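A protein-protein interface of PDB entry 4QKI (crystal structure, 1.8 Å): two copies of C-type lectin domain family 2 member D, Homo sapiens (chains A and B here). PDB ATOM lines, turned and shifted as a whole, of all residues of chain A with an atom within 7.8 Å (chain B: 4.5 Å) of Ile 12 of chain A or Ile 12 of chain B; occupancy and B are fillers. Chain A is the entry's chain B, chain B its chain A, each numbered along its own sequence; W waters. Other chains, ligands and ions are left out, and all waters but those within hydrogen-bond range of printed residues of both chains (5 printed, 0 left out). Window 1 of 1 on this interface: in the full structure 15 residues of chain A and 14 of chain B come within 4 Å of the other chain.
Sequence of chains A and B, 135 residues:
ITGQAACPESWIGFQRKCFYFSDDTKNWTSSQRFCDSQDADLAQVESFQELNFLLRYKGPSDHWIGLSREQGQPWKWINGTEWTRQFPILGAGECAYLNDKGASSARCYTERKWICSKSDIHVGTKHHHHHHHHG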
ATOM      1  N   CYS A   7      14.959  11.712   7.820  1.00  0.00           N
ATOM      2  CA  CYS A   7      14.538  10.820   6.745  1.00  0.00           C
ATOM      3  C   CYS A   7      15.143   9.436   6.897  1.00  0.00           C
ATOM      4  O   CYS A   7      16.220   9.247   7.413  1.00  0.00           O
ATOM      5  CB  CYS A   7      14.850  11.412   5.355  1.00  0.00           C
ATOM      6  SG  CYS A   7      14.054  12.990   4.936  1.00  0.00           S
ATOM      7  N   PRO A   8      14.447   8.424   6.388  1.00  0.00           N
ATOM      8  CA  PRO A   8      15.092   7.125   6.420  1.00  0.00           C
ATOM      9  C   PRO A   8      16.383   7.065   5.535  1.00  0.00           C
ATOM     10  O   PRO A   8      16.583   7.884   4.647  1.00  0.00           O
ATOM     11  CB  PRO A   8      13.990   6.165   5.938  1.00  0.00           C
ATOM     12  CG  PRO A   8      12.806   7.011   5.537  1.00  0.00           C
ATOM     13  CD  PRO A   8      13.180   8.454   5.633  1.00  0.00           C
ATOM     14  N   GLU A   9      17.263   6.142   5.843  1.00  0.00           N
ATOM     15  CA  GLU A   9      18.586   6.089   5.256  1.00  0.00           C
ATOM     16  C   GLU A   9      18.555   6.040   3.706  1.00  0.00           C
ATOM     17  O   GLU A   9      17.861   5.202   3.111  1.00  0.00           O
ATOM     18  CB  GLU A   9      19.318   4.896   5.824  1.00  0.00           C
ATOM     19  CG  GLU A   9      20.696   4.688   5.221  1.00  0.00           C
ATOM     20  CD  GLU A   9      20.711   3.656   4.111  1.00  0.00           C
ATOM     21  OE1 GLU A   9      19.934   2.673   4.202  1.00  0.00           O
ATOM     22  OE2 GLU A   9      21.515   3.812   3.155  1.00  0.00           O
ATOM     23  N   SER A  10      19.235   7.022   3.100  1.00  0.00           N
ATOM     24  CA  SER A  10      19.396   7.221   1.638  1.00  0.00           C
ATOM     25  C   SER A  10      18.249   7.961   0.937  1.00  0.00           C
ATOM     26  O   SER A  10      18.284   8.119  -0.318  1.00  0.00           O
ATOM     27  CB  SER A  10      19.739   5.901   0.921  1.00  0.00           C
ATOM     28  OG  SER A  10      21.106   5.576   1.170  1.00  0.00           O
ATOM     29  N   TRP A  11      17.251   8.431   1.707  1.00  0.00           N
ATOM     30  CA  TRP A  11      16.212   9.279   1.119  1.00  0.00           C
ATOM     31  C   TRP A  11      16.747  10.667   1.176  1.00  0.00           C
ATOM     32  O   TRP A  11      17.643  11.013   1.973  1.00  0.00           O
ATOM     33  CB  TRP A  11      14.833   9.189   1.836  1.00  0.00           C
ATOM     34  CG  TRP A  11      14.088   7.838   1.850  1.00  0.00           C
ATOM     35  CD1 TRP A  11      14.609   6.598   2.047  1.00  0.00           C
ATOM     36  CD2 TRP A  11      12.682   7.632   1.664  1.00  0.00           C
ATOM     37  NE1 TRP A  11      13.649   5.641   2.011  1.00  0.00           N
ATOM     38  CE2 TRP A  11      12.435   6.257   1.846  1.00  0.00           C
ATOM     39  CE3 TRP A  11      11.596   8.488   1.471  1.00  0.00           C
ATOM     40  CZ2 TRP A  11      11.170   5.703   1.699  1.00  0.00           C
ATOM     41  CZ3 TRP A  11      10.336   7.933   1.346  1.00  0.00           C
ATOM     42  CH2 TRP A  11      10.125   6.573   1.490  1.00  0.00           C
ATOM     43  N   ILE A  12      16.255  11.492   0.315  1.00  0.00           N
ATOM     44  CA  ILE A  12      16.814  12.771   0.158  1.00  0.00           C
ATOM     45  C   ILE A  12      15.812  13.682   0.854  1.00  0.00           C
ATOM     46  O   ILE A  12      14.581  13.589   0.618  1.00  0.00           O
ATOM     47  CB  ILE A  12      16.921  13.110  -1.322  1.00  0.00           C
ATOM     48  CG1 ILE A  12      17.606  11.969  -2.116  1.00  0.00           C
ATOM     49  CG2 ILE A  12      17.560  14.467  -1.521  1.00  0.00           C
ATOM     50  CD1 ILE A  12      18.901  11.388  -1.550  1.00  0.00           C
ATOM     51  N   GLY A  13      16.323  14.604   1.659  1.00  0.00           N
ATOM     52  CA  GLY A  13      15.470  15.488   2.385  1.00  0.00           C
ATOM     53  C   GLY A  13      15.368  16.786   1.676  1.00  0.00           C
ATOM     54  O   GLY A  13      16.374  17.302   1.224  1.00  0.00           O
ATOM     55  N   PHE A  14      14.150  17.318   1.555  1.00  0.00           N
ATOM     56  CA  PHE A  14      13.956  18.577   0.942  1.00  0.00           C
ATOM     57  C   PHE A  14      12.689  19.202   1.522  1.00  0.00           C
ATOM     58  O   PHE A  14      11.618  18.611   1.416  1.00  0.00           O
ATOM     59  CB  PHE A  14      13.816  18.414  -0.559  1.00  0.00           C
ATOM     60  CG  PHE A  14      13.723  19.697  -1.299  1.00  0.00           C
ATOM     61  CD1 PHE A  14      14.794  20.591  -1.296  1.00  0.00           C
ATOM     62  CD2 PHE A  14      12.572  20.031  -2.007  1.00  0.00           C
ATOM     63  CE1 PHE A  14      14.714  21.777  -1.983  1.00  0.00           C
ATOM     64  CE2 PHE A  14      12.499  21.232  -2.715  1.00  0.00           C
ATOM     65  CZ  PHE A  14      13.557  22.100  -2.705  1.00  0.00           C
ATOM     66  N   GLN A  15      12.815  20.413   2.051  1.00  0.00           N
ATOM     67  CA  GLN A  15      11.656  21.230   2.442  1.00  0.00           C
ATOM     68  C   GLN A  15      10.632  20.498   3.294  1.00  0.00           C
ATOM     69  O   GLN A  15       9.438  20.551   2.995  1.00  0.00           O
ATOM     70  CB  GLN A  15      10.946  21.765   1.213  1.00  0.00           C
ATOM     71  CG  GLN A  15      11.779  22.755   0.468  1.00  0.00           C
ATOM     72  CD  GLN A  15      10.980  23.795  -0.241  1.00  0.00           C
ATOM     73  OE1 GLN A  15       9.858  23.550  -0.699  1.00  0.00           O
ATOM     74  NE2 GLN A  15      11.551  24.989  -0.336  1.00  0.00           N
ATOM     75  N   ARG A  16      11.091  19.826   4.333  1.00  0.00           N
ATOM     76  CA  ARG A  16      10.224  19.082   5.291  1.00  0.00           C
ATOM     77  C   ARG A  16       9.620  17.768   4.759  1.00  0.00           C
ATOM     78  O   ARG A  16       8.760  17.164   5.413  1.00  0.00           O
ATOM     79  CB  ARG A  16       9.119  19.971   5.930  1.00  0.00           C
ATOM     80  CG  ARG A  16       9.621  21.225   6.663  1.00  0.00           C
ATOM     81  CD  ARG A  16      10.808  20.952   7.560  1.00  0.00           C
ATOM     82  NE  ARG A  16      10.581  19.967   8.629  1.00  0.00           N
ATOM     83  CZ  ARG A  16      10.206  20.227   9.887  1.00  0.00           C
ATOM     84  NH1 ARG A  16       9.963  21.467  10.305  1.00  0.00           N
ATOM     85  NH2 ARG A  16      10.054  19.220  10.742  1.00  0.00           N
ATOM     86  N   LYS A  17      10.099  17.301   3.600  1.00  0.00           N
ATOM     87  CA  LYS A  17       9.702  15.997   3.093  1.00  0.00           C
ATOM     88  C   LYS A  17      10.931  15.125   2.871  1.00  0.00           C
ATOM     89  O   LYS A  17      12.075  15.611   2.884  1.00  0.00           O
ATOM     90  CB  LYS A  17       8.949  16.165   1.787  1.00  0.00           C
ATOM     91  CG  LYS A  17       7.653  16.930   1.955  1.00  0.00           C
ATOM     92  CD  LYS A  17       6.862  16.921   0.661  1.00  0.00           C
ATOM     93  CE  LYS A  17       5.413  17.273   0.894  1.00  0.00           C
ATOM     94  NZ  LYS A  17       4.496  16.094   0.830  1.00  0.00           N
ATOM     95  N   CYS A  18      10.683  13.844   2.672  1.00  0.00           N
ATOM     96  CA  CYS A  18      11.723  12.892   2.296  1.00  0.00           C
ATOM     97  C   CYS A  18      11.319  12.225   0.995  1.00  0.00           C
ATOM     98  O   CYS A  18      10.155  11.804   0.828  1.00  0.00           O
ATOM     99  CB  CYS A  18      11.783  11.833   3.358  1.00  0.00           C
ATOM    100  SG  CYS A  18      12.016  12.576   4.994  1.00  0.00           S
ATOM    101  N   PHE A  19      12.312  12.023   0.132  1.00  0.00           N
ATOM    102  CA  PHE A  19      12.103  11.443  -1.176  1.00  0.00           C
ATOM    103  C   PHE A  19      12.952  10.194  -1.414  1.00  0.00           C
ATOM    104  O   PHE A  19      14.187  10.190  -1.144  1.00  0.00           O
ATOM    105  CB  PHE A  19      12.382  12.505  -2.194  1.00  0.00           C
ATOM    106  CG  PHE A  19      11.467  13.681  -2.107  1.00  0.00           C
ATOM    107  CD1 PHE A  19      11.787  14.746  -1.293  1.00  0.00           C
ATOM    108  CD2 PHE A  19      10.283  13.721  -2.801  1.00  0.00           C
ATOM    109  CE1 PHE A  19      10.931  15.827  -1.162  1.00  0.00           C
ATOM    110  CE2 PHE A  19       9.436  14.830  -2.697  1.00  0.00           C
ATOM    111  CZ  PHE A  19       9.762  15.863  -1.881  1.00  0.00           C
ATOM    112  N   TYR A  20      12.315   9.136  -1.933  1.00  0.00           N
ATOM    113  CA  TYR A  20      12.971   7.900  -2.292  1.00  0.00           C
ATOM    114  C   TYR A  20      13.028   7.795  -3.811  1.00  0.00           C
ATOM    115  O   TYR A  20      11.946   7.832  -4.475  1.00  0.00           O
ATOM    116  CB  TYR A  20      12.191   6.708  -1.765  1.00  0.00           C
ATOM    117  CG  TYR A  20      12.802   5.360  -2.089  1.00  0.00           C
ATOM    118  CD1 TYR A  20      13.823   4.837  -1.304  1.00  0.00           C
ATOM    119  CD2 TYR A  20      12.421   4.658  -3.254  1.00  0.00           C
ATOM    120  CE1 TYR A  20      14.407   3.609  -1.621  1.00  0.00           C
ATOM    121  CE2 TYR A  20      12.984   3.448  -3.586  1.00  0.00           C
ATOM    122  CZ  TYR A  20      13.978   2.928  -2.776  1.00  0.00           C
ATOM    123  OH  TYR A  20      14.517   1.718  -3.118  1.00  0.00           O
ATOM    124  N   PHE A  21      14.247   7.672  -4.359  1.00  0.00           N
ATOM    125  CA  PHE A  21      14.420   7.476  -5.799  1.00  0.00           C
ATOM    126  C   PHE A  21      14.865   6.038  -6.091  1.00  0.00           C
ATOM    127  O   PHE A  21      15.974   5.648  -5.644  1.00  0.00           O
ATOM    128  CB  PHE A  21      15.392   8.485  -6.431  1.00  0.00           C
ATOM    129  CG  PHE A  21      14.981   9.918  -6.295  1.00  0.00           C
ATOM    130  CD1 PHE A  21      15.072  10.600  -5.037  1.00  0.00           C
ATOM    131  CD2 PHE A  21      14.595  10.637  -7.388  1.00  0.00           C
ATOM    132  CE1 PHE A  21      14.741  11.938  -4.946  1.00  0.00           C
ATOM    133  CE2 PHE A  21      14.267  11.994  -7.267  1.00  0.00           C
ATOM    134  CZ  PHE A  21      14.321  12.619  -6.041  1.00  0.00           C
ATOM    135  N   PHE A  53      13.039  20.321  -8.387  1.00  0.00           N
ATOM    136  CA  PHE A  53      13.924  19.543  -7.513  1.00  0.00           C
ATOM    137  C   PHE A  53      13.991  18.010  -7.865  1.00  0.00           C
ATOM    138  O   PHE A  53      15.089  17.332  -7.825  1.00  0.00           O
ATOM    139  CB  PHE A  53      13.562  19.755  -6.030  1.00  0.00           C
ATOM    140  CG  PHE A  53      13.976  18.625  -5.136  1.00  0.00           C
ATOM    141  CD1 PHE A  53      15.270  18.515  -4.682  1.00  0.00           C
ATOM    142  CD2 PHE A  53      13.099  17.594  -4.826  1.00  0.00           C
ATOM    143  CE1 PHE A  53      15.683  17.471  -3.935  1.00  0.00           C
ATOM    144  CE2 PHE A  53      13.532  16.534  -4.056  1.00  0.00           C
ATOM    145  CZ  PHE A  53      14.819  16.473  -3.620  1.00  0.00           C
ATOM    146  N   LEU A  54      12.825  17.428  -8.154  1.00  0.00           N
ATOM    147  CA  LEU A  54      12.783  16.020  -8.525  1.00  0.00           C
ATOM    148  C   LEU A  54      13.514  15.843  -9.845  1.00  0.00           C
ATOM    149  O   LEU A  54      14.237  14.844 -10.029  1.00  0.00           O
ATOM    150  CB  LEU A  54      11.300  15.478  -8.595  1.00  0.00           C
ATOM    151  CG  LEU A  54      10.485  15.566  -7.322  1.00  0.00           C
ATOM    152  CD1 LEU A  54       9.038  15.079  -7.541  1.00  0.00           C
ATOM    153  CD2 LEU A  54      11.068  14.821  -6.161  1.00  0.00           C
ATOM    154  N   ARG A  56      15.937  17.598 -10.901  1.00  0.00           N
ATOM    155  CA  ARG A  56      17.388  17.765 -10.718  1.00  0.00           C
ATOM    156  C   ARG A  56      18.092  16.457 -10.325  1.00  0.00           C
ATOM    157  O   ARG A  56      19.177  16.158 -10.873  1.00  0.00           O
ATOM    158  CB  ARG A  56      17.719  18.896  -9.724  1.00  0.00           C
ATOM    159  CG  ARG A  56      19.216  19.153  -9.613  1.00  0.00           C
ATOM    160  CD  ARG A  56      19.528  20.483  -8.948  1.00  0.00           C
ATOM    161  NE  ARG A  56      20.975  20.703  -8.842  1.00  0.00           N
ATOM    162  CZ  ARG A  56      21.536  21.859  -8.471  1.00  0.00           C
ATOM    163  NH1 ARG A  56      22.858  21.943  -8.346  1.00  0.00           N
ATOM    164  NH2 ARG A  56      20.789  22.909  -8.170  1.00  0.00           N
ATOM    165  N   TYR A  57      17.501  15.696  -9.400  1.00  0.00           N
ATOM    166  CA  TYR A  57      18.099  14.511  -8.875  1.00  0.00           C
ATOM    167  C   TYR A  57      17.790  13.239  -9.665  1.00  0.00           C
ATOM    168  O   TYR A  57      18.487  12.239  -9.589  1.00  0.00           O
ATOM    169  CB  TYR A  57      17.674  14.314  -7.454  1.00  0.00           C
ATOM    170  CG  TYR A  57      18.465  13.240  -6.744  1.00  0.00           C
ATOM    171  CD1 TYR A  57      19.835  13.443  -6.414  1.00  0.00           C
ATOM    172  CD2 TYR A  57      17.900  12.029  -6.419  1.00  0.00           C
ATOM    173  CE1 TYR A  57      20.553  12.497  -5.755  1.00  0.00           C
ATOM    174  CE2 TYR A  57      18.645  11.055  -5.777  1.00  0.00           C
ATOM    175  CZ  TYR A  57      19.975  11.322  -5.434  1.00  0.00           C
ATOM    176  OH  TYR A  57      20.707  10.363  -4.813  1.00  0.00           O
ATOM    177  N   CYS A 116       9.054   7.916  -4.224  1.00  0.00           N
ATOM    178  CA  CYS A 116       8.141   8.037  -3.094  1.00  0.00           C
ATOM    179  C   CYS A 116       8.362   9.375  -2.365  1.00  0.00           C
ATOM    180  O   CYS A 116       9.488   9.896  -2.301  1.00  0.00           O
ATOM    181  CB  CYS A 116       8.337   6.898  -2.059  1.00  0.00           C
ATOM    182  SG  CYS A 116       8.336   5.165  -2.577  1.00  0.00           S
ATOM    183  N   SER A 117       7.332   9.899  -1.697  1.00  0.00           N
ATOM    184  CA  SER A 117       7.546  11.001  -0.771  1.00  0.00           C
ATOM    185  C   SER A 117       6.715  10.843   0.459  1.00  0.00           C
ATOM    186  O   SER A 117       5.675  10.142   0.464  1.00  0.00           O
ATOM    187  CB  SER A 117       7.304  12.381  -1.402  1.00  0.00           C
ATOM    188  OG  SER A 117       5.974  12.561  -1.807  1.00  0.00           O
ATOM    189  N   LYS A 118       7.189  11.463   1.536  1.00  0.00           N
ATOM    190  CA  LYS A 118       6.401  11.534   2.811  1.00  0.00           C
ATOM    191  C   LYS A 118       6.926  12.694   3.601  1.00  0.00           C
ATOM    192  O   LYS A 118       7.992  13.235   3.280  1.00  0.00           O
ATOM    193  CB  LYS A 118       6.505  10.278   3.649  1.00  0.00           C
ATOM    194  CG  LYS A 118       7.918   9.818   3.941  1.00  0.00           C
ATOM    195  CD  LYS A 118       7.903   8.903   5.124  1.00  0.00           C
ATOM    196  CE  LYS A 118       9.174   8.118   5.206  1.00  0.00           C
ATOM    197  NZ  LYS A 118       9.043   7.083   6.257  1.00  0.00           N
ATOM    198  N   SER B  10      16.077  25.208   1.707  1.00  0.00           N
ATOM    199  CA  SER B  10      16.773  25.075   0.423  1.00  0.00           C
ATOM    200  C   SER B  10      18.079  24.256   0.489  1.00  0.00           C
ATOM    201  O   SER B  10      18.758  24.130  -0.529  1.00  0.00           O
ATOM    202  CB  SER B  10      17.052  26.429  -0.218  1.00  0.00           C
ATOM    203  OG  SER B  10      18.197  27.034   0.351  1.00  0.00           O
ATOM    204  N   TRP B  11      18.462  23.734   1.653  1.00  0.00           N
ATOM    205  CA  TRP B  11      19.586  22.797   1.667  1.00  0.00           C
ATOM    206  C   TRP B  11      18.970  21.426   1.432  1.00  0.00           C
ATOM    207  O   TRP B  11      17.773  21.214   1.727  1.00  0.00           O
ATOM    208  CB  TRP B  11      20.361  22.867   2.994  1.00  0.00           C
ATOM    209  CG  TRP B  11      21.115  24.129   3.176  1.00  0.00           C
ATOM    210  CD1 TRP B  11      20.669  25.446   2.951  1.00  0.00           C
ATOM    211  CD2 TRP B  11      22.440  24.255   3.664  1.00  0.00           C
ATOM    212  NE1 TRP B  11      21.656  26.342   3.273  1.00  0.00           N
ATOM    213  CE2 TRP B  11      22.751  25.650   3.715  1.00  0.00           C
ATOM    214  CE3 TRP B  11      23.407  23.338   4.052  1.00  0.00           C
ATOM    215  CZ2 TRP B  11      23.992  26.124   4.128  1.00  0.00           C
ATOM    216  CZ3 TRP B  11      24.646  23.822   4.482  1.00  0.00           C
ATOM    217  CH2 TRP B  11      24.918  25.203   4.524  1.00  0.00           C
ATOM    218  N   ILE B  12      19.787  20.479   0.976  1.00  0.00           N
ATOM    219  CA  ILE B  12      19.380  19.145   0.674  1.00  0.00           C
ATOM    220  C   ILE B  12      19.927  18.191   1.704  1.00  0.00           C
ATOM    221  O   ILE B  12      21.117  18.197   1.980  1.00  0.00           O
ATOM    222  CB  ILE B  12      19.863  18.679  -0.729  1.00  0.00           C
ATOM    223  CG1 ILE B  12      19.560  19.726  -1.798  1.00  0.00           C
ATOM    224  CG2 ILE B  12      19.279  17.334  -1.080  1.00  0.00           C
ATOM    225  CD1 ILE B  12      18.115  20.197  -1.915  1.00  0.00           C
ATOM    226  N   GLY B  13      19.027  17.391   2.306  1.00  0.00           N
ATOM    227  CA  GLY B  13      19.408  16.370   3.239  1.00  0.00           C
ATOM    228  C   GLY B  13      19.785  15.046   2.672  1.00  0.00           C
ATOM    229  O   GLY B  13      19.083  14.521   1.768  1.00  0.00           O
ATOM    230  N   PHE B  14      20.875  14.481   3.212  1.00  0.00           N
ATOM    231  CA  PHE B  14      21.372  13.144   2.826  1.00  0.00           C
ATOM    232  C   PHE B  14      22.182  12.537   3.976  1.00  0.00           C
ATOM    233  O   PHE B  14      23.168  13.111   4.408  1.00  0.00           O
ATOM    234  CB  PHE B  14      22.194  13.218   1.535  1.00  0.00           C
ATOM    235  CG  PHE B  14      22.705  11.862   1.038  1.00  0.00           C
ATOM    236  CD1 PHE B  14      21.816  10.928   0.440  1.00  0.00           C
ATOM    237  CD2 PHE B  14      24.020  11.475   1.256  1.00  0.00           C
ATOM    238  CE1 PHE B  14      22.277   9.686  -0.009  1.00  0.00           C
ATOM    239  CE2 PHE B  14      24.476  10.195   0.829  1.00  0.00           C
ATOM    240  CZ  PHE B  14      23.590   9.317   0.211  1.00  0.00           C
ATOM    241  N   LYS B  17      23.651  14.602   6.979  1.00  0.00           N
ATOM    242  CA  LYS B  17      24.163  15.927   6.606  1.00  0.00           C
ATOM    243  C   LYS B  17      23.197  16.714   5.776  1.00  0.00           C
ATOM    244  O   LYS B  17      22.251  16.157   5.252  1.00  0.00           O
ATOM    245  CB  LYS B  17      25.483  15.812   5.831  1.00  0.00           C
ATOM    246  CG  LYS B  17      26.594  15.164   6.612  1.00  0.00           C
ATOM    247  CD  LYS B  17      27.803  14.928   5.706  1.00  0.00           C
ATOM    248  CE  LYS B  17      29.033  14.569   6.495  1.00  0.00           C
ATOM    249  NZ  LYS B  17      30.300  14.592   5.625  1.00  0.00           N
ATOM    250  N   CYS B  18      23.487  18.019   5.645  1.00  0.00           N
ATOM    251  CA  CYS B  18      22.733  18.992   4.913  1.00  0.00           C
ATOM    252  C   CYS B  18      23.720  19.619   3.961  1.00  0.00           C
ATOM    253  O   CYS B  18      24.802  20.038   4.399  1.00  0.00           O
ATOM    254  CB  CYS B  18      22.244  20.073   5.872  1.00  0.00           C
ATOM    255  SG  CYS B  18      21.208  19.464   7.217  1.00  0.00           S
ATOM    256  N   PHE B  19      23.349  19.691   2.695  1.00  0.00           N
ATOM    257  CA  PHE B  19      24.189  20.197   1.617  1.00  0.00           C
ATOM    258  C   PHE B  19      23.574  21.398   0.909  1.00  0.00           C
ATOM    259  O   PHE B  19      22.365  21.436   0.601  1.00  0.00           O
ATOM    260  CB  PHE B  19      24.441  19.110   0.582  1.00  0.00           C
ATOM    261  CG  PHE B  19      25.212  17.940   1.083  1.00  0.00           C
ATOM    262  CD1 PHE B  19      26.584  17.980   1.110  1.00  0.00           C
ATOM    263  CD2 PHE B  19      24.563  16.813   1.610  1.00  0.00           C
ATOM    264  CE1 PHE B  19      27.317  16.904   1.576  1.00  0.00           C
ATOM    265  CE2 PHE B  19      25.293  15.744   2.097  1.00  0.00           C
ATOM    266  CZ  PHE B  19      26.691  15.798   2.079  1.00  0.00           C
ATOM    267  N   PHE B  21      24.113  23.711  -2.564  1.00  0.00           N
ATOM    268  CA  PHE B  21      24.662  23.765  -3.922  1.00  0.00           C
ATOM    269  C   PHE B  21      24.477  25.164  -4.433  1.00  0.00           C
ATOM    270  O   PHE B  21      23.336  25.671  -4.533  1.00  0.00           O
ATOM    271  CB  PHE B  21      23.982  22.758  -4.864  1.00  0.00           C
ATOM    272  CG  PHE B  21      24.133  21.353  -4.438  1.00  0.00           C
ATOM    273  CD1 PHE B  21      23.328  20.805  -3.419  1.00  0.00           C
ATOM    274  CD2 PHE B  21      25.065  20.536  -5.057  1.00  0.00           C
ATOM    275  CE1 PHE B  21      23.493  19.497  -3.039  1.00  0.00           C
ATOM    276  CE2 PHE B  21      25.250  19.229  -4.646  1.00  0.00           C
ATOM    277  CZ  PHE B  21      24.458  18.694  -3.643  1.00  0.00           C
ATOM    278  N   PHE B  53      26.068  10.795  -4.246  1.00  0.00           N
ATOM    279  CA  PHE B  53      24.953  11.747  -4.094  1.00  0.00           C
ATOM    280  C   PHE B  53      25.283  13.115  -4.684  1.00  0.00           C
ATOM    281  O   PHE B  53      24.554  13.699  -5.512  1.00  0.00           O
ATOM    282  CB  PHE B  53      24.617  11.907  -2.597  1.00  0.00           C
ATOM    283  CG  PHE B  53      23.726  13.110  -2.330  1.00  0.00           C
ATOM    284  CD1 PHE B  53      22.406  13.094  -2.708  1.00  0.00           C
ATOM    285  CD2 PHE B  53      24.226  14.239  -1.710  1.00  0.00           C
ATOM    286  CE1 PHE B  53      21.579  14.186  -2.497  1.00  0.00           C
ATOM    287  CE2 PHE B  53      23.420  15.347  -1.510  1.00  0.00           C
ATOM    288  CZ  PHE B  53      22.074  15.316  -1.883  1.00  0.00           C
ATOM    289  N   TYR B  57      23.322  14.940  -7.827  1.00  0.00           N
ATOM    290  CA  TYR B  57      22.575  16.195  -7.657  1.00  0.00           C
ATOM    291  C   TYR B  57      23.125  17.419  -8.380  1.00  0.00           C
ATOM    292  O   TYR B  57      22.375  18.226  -8.846  1.00  0.00           O
ATOM    293  CB  TYR B  57      22.331  16.510  -6.180  1.00  0.00           C
ATOM    294  CG  TYR B  57      21.276  17.574  -5.976  1.00  0.00           C
ATOM    295  CD1 TYR B  57      19.939  17.243  -5.827  1.00  0.00           C
ATOM    296  CD2 TYR B  57      21.617  18.905  -5.877  1.00  0.00           C
ATOM    297  CE1 TYR B  57      18.980  18.217  -5.645  1.00  0.00           C
ATOM    298  CE2 TYR B  57      20.657  19.872  -5.709  1.00  0.00           C
ATOM    299  CZ  TYR B  57      19.346  19.522  -5.599  1.00  0.00           C
ATOM    300  OH  TYR B  57      18.394  20.519  -5.446  1.00  0.00           O
HETATM  301  O   HOH W   1      21.738  25.179  -6.951  1.00  0.00           O
HETATM  302  O   HOH W   2      16.381  19.548   3.810  1.00  0.00           O
HETATM  303  O   HOH W   3      23.253   9.086  -5.069  1.00  0.00           O
HETATM  304  O   HOH W   4      15.351  21.727   2.413  1.00  0.00           O
HETATM  305  O   HOH W   5      17.920  12.780   4.412  1.00  0.00           O
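The backbone carbonyl oxygen of Phe 19 of chain B is in hydrogen-bond range of the backbone NH of Ile 12 of chain B (2.8 Å). The backbone carbonyl oxygen of Ile 12 of chain A lies within hydrogen-bond range of the backbone NH of Phe 19 of chain A. SG of Cys 18 of chain A forms a disulfide with SG of Cys 7 of chain A (2.1 Å).
Water W1 bridges the guanidinium group of Arg 56 of chain A (2.7 Å) and the backbone carbonyl oxygen of Phe 21 of chain B (2.9 Å). Water W3 bridges the side-chain hydroxyl (OH) of Tyr 57 of chain A and the backbone NH (N) of Phe 53 of chain B. Water W5 bridges O of Trp 11 of chain A (3.0 Å) and O of Gly 13 of chain B (3.4 Å).
Trp 11 of chain A touches Gly 13 of chain B, but with the chains exchanged Gly 13 of chain A does not touch Trp 11 of chain B (4.2 Å). Ile 12 of chain A touches Gly 13 of chain B, and with the chains exchanged Gly 13 of chain A touches Ile 12 of chain B. Tyr 57 of chain B touches its own counterpart, Tyr 57 of chain A. 11 positions are printed for both chains.
Hydrophobic or aromatic side chains of chain A that line the printed part of chain B: Ile 12, Phe 14, Phe 53 and Tyr 57. Along chain B the printed residues that touch a printed residue of chain A span positions 12 to 57. Among the printed residues, no Asp or Glu carboxylate lies within 4 Å of a Lys or Arg side-chain nitrogen of the other chain.
Among the printed residues, pairs that only touch across the chains: Ile 12 of chain A with Gly 13 of chain B, Ile 12 of chain A with Ile 12 of chain B, Phe 14 of chain A with Ile 12 of chain B, Ile 12 of chain A with Phe 14 of chain B, Gly 13 of chain A with Ile 12 of chain B, Tyr 57 of chain A with Phe 53 of chain B, Arg 56 of chain A with Phe 21 of chain B, Phe 53 of chain A with Tyr 57 of chain B, Trp 11 of chain A with Gly 13 of chain B, Tyr 57 of chain A with Tyr 57 of chain B and Ile 12 of chain A with Phe 53 of chain B.
Of the printed residues of chain B, Ile 12 of chain A touches Ile 12, Gly 13, Phe 14 and Phe 53. Ile 12 of chain B touches just these residues of chain A: Ile 12, Gly 13 and Phe 14. Printed residues of chain B within 4 Å of Phe 53 of chain A: Tyr 57 (3.8 Å). Of the printed residues of chain A, Phe 14 of chain B touches Ile 12. Printed residues of chain A within 4 Å of Phe 53 of chain B: Ile 12 (3.99 Å) and Tyr 57 (3.6 Å). Cys 18 of chain B touches none of the printed residues of chain A. The nearest residue of chain A that does not touch Ile 12 of chain B is Phe 53 of chain A (4.2 Å). The nearest printed residue of chain B that does not touch Gly 13 of chain A is Trp 11 of chain B (4.2 Å).
The backbone NH (N) of Gly 13 of chain A sits at hydrogen-bond distance from the backbone carbonyl oxygen (O) of Gly 13 of chain B, 2.8 Å away. The guanidinium group (NE) of Arg 56 of chain A sits at hydrogen-bond distance from the backbone carbonyl oxygen (O) of Tyr 57 of chain B, at 2.8 Å.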
